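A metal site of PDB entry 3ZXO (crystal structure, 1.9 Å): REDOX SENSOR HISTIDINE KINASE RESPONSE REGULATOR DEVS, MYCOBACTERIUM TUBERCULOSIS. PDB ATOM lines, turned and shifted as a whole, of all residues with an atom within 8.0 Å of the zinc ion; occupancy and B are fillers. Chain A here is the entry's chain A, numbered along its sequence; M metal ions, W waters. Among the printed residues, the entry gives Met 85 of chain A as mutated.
The side-chain carboxylate (OD1) of Asp 80 sits at hydrogen-bond distance from the backbone NH (N) of Gly 82, at 2.8 Å. The backbone NH of Asp 80 sits at hydrogen-bond distance from the backbone carbonyl oxygen of Thr 119, 2.8 Å away. NE2 of His 58 sits close to O of Val 56, 3.5 Å away. A ring nitrogen (ND1) of His 58 lies within hydrogen-bond range of the backbone carbonyl oxygen of Arg 83, at 2.8 Å. The side-chain carboxylate of Glu 88 sits close to the backbone NH of Val 56 (2.8 Å).
Val 56 touches the zinc ion (O to ZN, 3.6 Å). Of the 22 residues printed, 4 come within 4 Å of the zinc ion. The nearest printed residue that does not touch the zinc ion is Phe 89 (4.3 Å).
The zinc ion is bound by OD2 of Asp 80, NE2 of His 58, water W1 and OE2 of Glu 88. The zinc ion has four donor atoms within binding distance. Slightly farther from the zinc ion lies OE1 of Glu 88 (2.7 Å).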
ATOM      1  N   LEU A  23      -7.486  11.540  17.945  1.00  0.00           N
ATOM      2  CA  LEU A  23      -6.231  11.802  17.217  1.00  0.00           C
ATOM      3  C   LEU A  23      -5.472  12.957  17.828  1.00  0.00           C
ATOM      4  O   LEU A  23      -6.090  13.859  18.356  1.00  0.00           O
ATOM      5  CB  LEU A  23      -6.525  12.144  15.740  1.00  0.00           C
ATOM      6  CG  LEU A  23      -7.417  11.107  15.047  1.00  0.00           C
ATOM      7  CD1 LEU A  23      -7.787  11.533  13.608  1.00  0.00           C
ATOM      8  CD2 LEU A  23      -6.769   9.657  15.080  1.00  0.00           C
ATOM      9  N   ALA A  51      -9.962  16.947   4.651  1.00  0.00           N
ATOM     10  CA  ALA A  51      -8.842  16.017   4.972  1.00  0.00           C
ATOM     11  C   ALA A  51      -8.960  15.570   6.420  1.00  0.00           C
ATOM     12  O   ALA A  51      -8.939  14.371   6.728  1.00  0.00           O
ATOM     13  CB  ALA A  51      -7.492  16.718   4.739  1.00  0.00           C
ATOM     14  N   VAL A  52      -9.125  16.535   7.301  1.00  0.00           N
ATOM     15  CA  VAL A  52      -9.141  16.262   8.727  1.00  0.00           C
ATOM     16  C   VAL A  52     -10.403  15.477   9.135  1.00  0.00           C
ATOM     17  O   VAL A  52     -10.342  14.564   9.966  1.00  0.00           O
ATOM     18  CB  VAL A  52      -9.008  17.560   9.530  1.00  0.00           C
ATOM     19  CG1 VAL A  52      -9.341  17.350  10.982  1.00  0.00           C
ATOM     20  CG2 VAL A  52      -7.573  18.062   9.392  1.00  0.00           C
ATOM     21  N   ASN A  54     -12.110  13.439   7.362  1.00  0.00           N
ATOM     22  CA  ASN A  54     -12.024  12.077   6.854  1.00  0.00           C
ATOM     23  C   ASN A  54     -11.029  11.165   7.589  1.00  0.00           C
ATOM     24  O   ASN A  54     -11.061   9.967   7.390  1.00  0.00           O
ATOM     25  CB  ASN A  54     -11.799  12.055   5.338  1.00  0.00           C
ATOM     26  CG  ASN A  54     -13.095  12.342   4.594  1.00  0.00           C
ATOM     27  OD1 ASN A  54     -13.855  11.412   4.318  1.00  0.00           O
ATOM     28  ND2 ASN A  54     -13.442  13.640   4.433  1.00  0.00           N
ATOM     29  N   ALA A  55     -10.178  11.742   8.433  1.00  0.00           N
ATOM     30  CA  ALA A  55      -9.232  10.922   9.231  1.00  0.00           C
ATOM     31  C   ALA A  55      -9.996  10.104  10.280  1.00  0.00           C
ATOM     32  O   ALA A  55     -10.938  10.591  10.905  1.00  0.00           O
ATOM     33  CB  ALA A  55      -8.182  11.823   9.937  1.00  0.00           C
ATOM     34  N   VAL A  56      -9.570   8.872  10.518  1.00  0.00           N
ATOM     35  CA  VAL A  56     -10.280   8.009  11.446  1.00  0.00           C
ATOM     36  C   VAL A  56      -9.302   7.568  12.548  1.00  0.00           C
ATOM     37  O   VAL A  56      -8.096   7.751  12.416  1.00  0.00           O
ATOM     38  CB  VAL A  56     -10.893   6.753  10.745  1.00  0.00           C
ATOM     39  CG1 VAL A  56     -11.916   7.168   9.680  1.00  0.00           C
ATOM     40  CG2 VAL A  56      -9.791   5.888  10.134  1.00  0.00           C
ATOM     41  N   ARG A  57      -9.827   7.050  13.644  1.00  0.00           N
ATOM     42  CA  ARG A  57      -8.966   6.418  14.666  1.00  0.00           C
ATOM     43  C   ARG A  57      -8.270   5.178  14.132  1.00  0.00           C
ATOM     44  O   ARG A  57      -8.836   4.415  13.370  1.00  0.00           O
ATOM     45  CB  ARG A  57      -9.797   5.972  15.870  1.00  0.00           C
ATOM     46  CG  ARG A  57     -10.206   7.097  16.732  1.00  0.00           C
ATOM     47  CD  ARG A  57     -10.903   6.635  17.996  1.00  0.00           C
ATOM     48  NE  ARG A  57     -11.562   7.795  18.592  1.00  0.00           N
ATOM     49  CZ  ARG A  57     -12.005   7.870  19.846  1.00  0.00           C
ATOM     50  NH1 ARG A  57     -11.854   6.846  20.684  1.00  0.00           N
ATOM     51  NH2 ARG A  57     -12.588   8.989  20.261  1.00  0.00           N
ATOM     52  N   HIS A  58      -7.032   4.978  14.556  1.00  0.00           N
ATOM     53  CA  HIS A  58      -6.256   3.836  14.153  1.00  0.00           C
ATOM     54  C   HIS A  58      -6.030   2.877  15.354  1.00  0.00           C
ATOM     55  O   HIS A  58      -6.328   3.229  16.507  1.00  0.00           O
ATOM     56  CB  HIS A  58      -4.935   4.321  13.511  1.00  0.00           C
ATOM     57  CG  HIS A  58      -5.130   5.006  12.200  1.00  0.00           C
ATOM     58  ND1 HIS A  58      -5.094   4.325  10.993  1.00  0.00           N
ATOM     59  CD2 HIS A  58      -5.373   6.299  11.886  1.00  0.00           C
ATOM     60  CE1 HIS A  58      -5.323   5.182  10.001  1.00  0.00           C
ATOM     61  NE2 HIS A  58      -5.498   6.384  10.523  1.00  0.00           N
ATOM     62  N   SER A  62      -2.044   7.970  16.979  1.00  0.00           N
ATOM     63  CA  SER A  62      -1.606   8.531  15.689  1.00  0.00           C
ATOM     64  C   SER A  62      -1.782  10.040  15.691  1.00  0.00           C
ATOM     65  O   SER A  62      -2.558  10.584  16.501  1.00  0.00           O
ATOM     66  CB  SER A  62      -2.371   7.876  14.518  1.00  0.00           C
ATOM     67  OG  SER A  62      -3.757   8.207  14.522  1.00  0.00           O
ATOM     68  N   THR A  63      -1.053  10.706  14.795  1.00  0.00           N
ATOM     69  CA  THR A  63      -1.082  12.139  14.703  1.00  0.00           C
ATOM     70  C   THR A  63      -1.420  12.513  13.269  1.00  0.00           C
ATOM     71  O   THR A  63      -0.935  11.852  12.334  1.00  0.00           O
ATOM     72  CB  THR A  63       0.299  12.760  15.080  1.00  0.00           C
ATOM     73  OG1 THR A  63       0.587  12.420  16.431  1.00  0.00           O
ATOM     74  CG2 THR A  63       0.305  14.270  14.974  1.00  0.00           C
ATOM     75  N   LEU A  64      -2.245  13.545  13.098  1.00  0.00           N
ATOM     76  CA  LEU A  64      -2.349  14.208  11.805  1.00  0.00           C
ATOM     77  C   LEU A  64      -1.532  15.458  11.885  1.00  0.00           C
ATOM     78  O   LEU A  64      -1.796  16.313  12.755  1.00  0.00           O
ATOM     79  CB  LEU A  64      -3.776  14.677  11.505  1.00  0.00           C
ATOM     80  CG  LEU A  64      -4.865  13.700  11.146  1.00  0.00           C
ATOM     81  CD1 LEU A  64      -6.192  14.538  11.057  1.00  0.00           C
ATOM     82  CD2 LEU A  64      -4.529  13.010   9.833  1.00  0.00           C
ATOM     83  N   THR A  79      -0.209  14.859   6.800  1.00  0.00           N
ATOM     84  CA  THR A  79       0.487  13.582   6.978  1.00  0.00           C
ATOM     85  C   THR A  79      -0.166  12.819   8.130  1.00  0.00           C
ATOM     86  O   THR A  79      -0.386  13.381   9.218  1.00  0.00           O
ATOM     87  CB  THR A  79       1.992  13.802   7.255  1.00  0.00           C
ATOM     88  OG1 THR A  79       2.558  14.464   6.124  1.00  0.00           O
ATOM     89  CG2 THR A  79       2.713  12.511   7.372  1.00  0.00           C
ATOM     90  N   ASP A  80      -0.486  11.548   7.887  1.00  0.00           N
ATOM     91  CA  ASP A  80      -1.188  10.753   8.867  1.00  0.00           C
ATOM     92  C   ASP A  80      -0.270   9.584   9.104  1.00  0.00           C
ATOM     93  O   ASP A  80       0.057   8.847   8.159  1.00  0.00           O
ATOM     94  CB  ASP A  80      -2.532  10.306   8.258  1.00  0.00           C
ATOM     95  CG  ASP A  80      -3.323   9.420   9.152  1.00  0.00           C
ATOM     96  OD1 ASP A  80      -2.847   9.061  10.249  1.00  0.00           O
ATOM     97  OD2 ASP A  80      -4.463   9.057   8.778  1.00  0.00           O
ATOM     98  N   ASN A  81       0.201   9.410  10.339  1.00  0.00           N
ATOM     99  CA  ASN A  81       1.098   8.272  10.600  1.00  0.00           C
ATOM    100  C   ASN A  81       0.343   7.036  11.068  1.00  0.00           C
ATOM    101  O   ASN A  81       0.960   6.049  11.509  1.00  0.00           O
ATOM    102  CB  ASN A  81       2.239   8.666  11.537  1.00  0.00           C
ATOM    103  CG  ASN A  81       1.788   8.873  12.980  1.00  0.00           C
ATOM    104  OD1 ASN A  81       0.592   9.009  13.257  1.00  0.00           O
ATOM    105  ND2 ASN A  81       2.746   8.873  13.910  1.00  0.00           N
ATOM    106  N   GLY A  82      -0.993   7.068  10.973  1.00  0.00           N
ATOM    107  CA  GLY A  82      -1.811   5.934  11.333  1.00  0.00           C
ATOM    108  C   GLY A  82      -1.717   4.834  10.314  1.00  0.00           C
ATOM    109  O   GLY A  82      -1.672   5.094   9.125  1.00  0.00           O
ATOM    110  N   ARG A  83      -1.743   3.574  10.745  1.00  0.00           N
ATOM    111  CA  ARG A  83      -1.588   2.459   9.809  1.00  0.00           C
ATOM    112  C   ARG A  83      -2.910   1.752   9.516  1.00  0.00           C
ATOM    113  O   ARG A  83      -3.876   1.870  10.278  1.00  0.00           O
ATOM    114  CB  ARG A  83      -0.552   1.463  10.363  1.00  0.00           C
ATOM    115  CG  ARG A  83       0.625   2.178  11.075  1.00  0.00           C
ATOM    116  CD  ARG A  83       1.543   1.226  11.777  1.00  0.00           C
ATOM    117  NE  ARG A  83       2.199   0.369  10.799  1.00  0.00           N
ATOM    118  CZ  ARG A  83       3.336   0.668  10.162  1.00  0.00           C
ATOM    119  NH1 ARG A  83       3.981   1.802  10.408  1.00  0.00           N
ATOM    120  NH2 ARG A  83       3.841  -0.195   9.300  1.00  0.00           N
ATOM    121  N   GLY A  84      -2.947   0.970   8.444  1.00  0.00           N
ATOM    122  CA  GLY A  84      -4.154   0.205   8.112  1.00  0.00           C
ATOM    123  C   GLY A  84      -5.233   1.157   7.620  1.00  0.00           C
ATOM    124  O   GLY A  84      -4.923   2.275   7.126  1.00  0.00           O
ATOM    125  N   MET A  85      -6.480   0.754   7.779  1.00  0.00           N
ATOM    126  CA  MET A  85      -7.644   1.529   7.301  1.00  0.00           C
ATOM    127  C   MET A  85      -7.544   1.959   5.800  1.00  0.00           C
ATOM    128  O   MET A  85      -7.479   3.165   5.501  1.00  0.00           O
ATOM    129  CB  MET A  85      -7.878   2.745   8.226  1.00  0.00           C
ATOM    130  CG  MET A  85      -7.896   2.444   9.722  1.00  0.00           C
ATOM    131  SD  MET A  85      -9.326   1.122  10.141  1.00  0.00           S
ATOM    132  CE  MET A  85     -10.924   2.158   9.863  1.00  0.00           C
ATOM    133  N   GLU A  88      -9.689   4.672   4.396  1.00  0.00           N
ATOM    134  CA  GLU A  88      -9.587   6.034   4.923  1.00  0.00           C
ATOM    135  C   GLU A  88      -9.204   6.981   3.780  1.00  0.00           C
ATOM    136  O   GLU A  88      -8.331   6.659   2.975  1.00  0.00           O
ATOM    137  CB  GLU A  88      -8.493   6.101   5.989  1.00  0.00           C
ATOM    138  CG  GLU A  88      -8.466   7.393   6.753  1.00  0.00           C
ATOM    139  CD  GLU A  88      -7.331   7.439   7.767  1.00  0.00           C
ATOM    140  OE1 GLU A  88      -6.271   6.855   7.480  1.00  0.00           O
ATOM    141  OE2 GLU A  88      -7.485   8.102   8.805  1.00  0.00           O
ATOM    142  N   PHE A  89      -9.862   8.140   3.744  1.00  0.00           N
ATOM    143  CA  PHE A  89      -9.671   9.131   2.699  1.00  0.00           C
ATOM    144  C   PHE A  89     -10.106   8.777   1.266  1.00  0.00           C
ATOM    145  O   PHE A  89      -9.782   9.545   0.342  1.00  0.00           O
ATOM    146  CB  PHE A  89      -8.208   9.635   2.627  1.00  0.00           C
ATOM    147  CG  PHE A  89      -7.605  10.024   3.965  1.00  0.00           C
ATOM    148  CD1 PHE A  89      -8.084  11.112   4.668  1.00  0.00           C
ATOM    149  CD2 PHE A  89      -6.512   9.311   4.473  1.00  0.00           C
ATOM    150  CE1 PHE A  89      -7.544  11.496   5.886  1.00  0.00           C
ATOM    151  CE2 PHE A  89      -5.953   9.670   5.725  1.00  0.00           C
ATOM    152  CZ  PHE A  89      -6.463  10.770   6.427  1.00  0.00           C
ATOM    153  N   GLY A 118       1.199   4.758   6.633  1.00  0.00           N
ATOM    154  CA  GLY A 118       1.066   6.190   6.759  1.00  0.00           C
ATOM    155  C   GLY A 118       0.669   6.737   5.415  1.00  0.00           C
ATOM    156  O   GLY A 118       0.924   6.137   4.385  1.00  0.00           O
ATOM    157  N   THR A 119       0.011   7.891   5.444  1.00  0.00           N
ATOM    158  CA  THR A 119      -0.630   8.419   4.260  1.00  0.00           C
ATOM    159  C   THR A 119      -0.324   9.906   4.196  1.00  0.00           C
ATOM    160  O   THR A 119      -0.329  10.583   5.225  1.00  0.00           O
ATOM    161  CB  THR A 119      -2.162   8.207   4.297  1.00  0.00           C
ATOM    162  OG1 THR A 119      -2.439   6.817   4.470  1.00  0.00           O
ATOM    163  CG2 THR A 119      -2.787   8.636   3.013  1.00  0.00           C
HETATM  164 ZN    ZN M   1      -5.727   8.148   9.747  1.00  0.00          ZN
HETATM  165  O   HOH W   1      -6.273   9.305  11.223  1.00  0.00           O
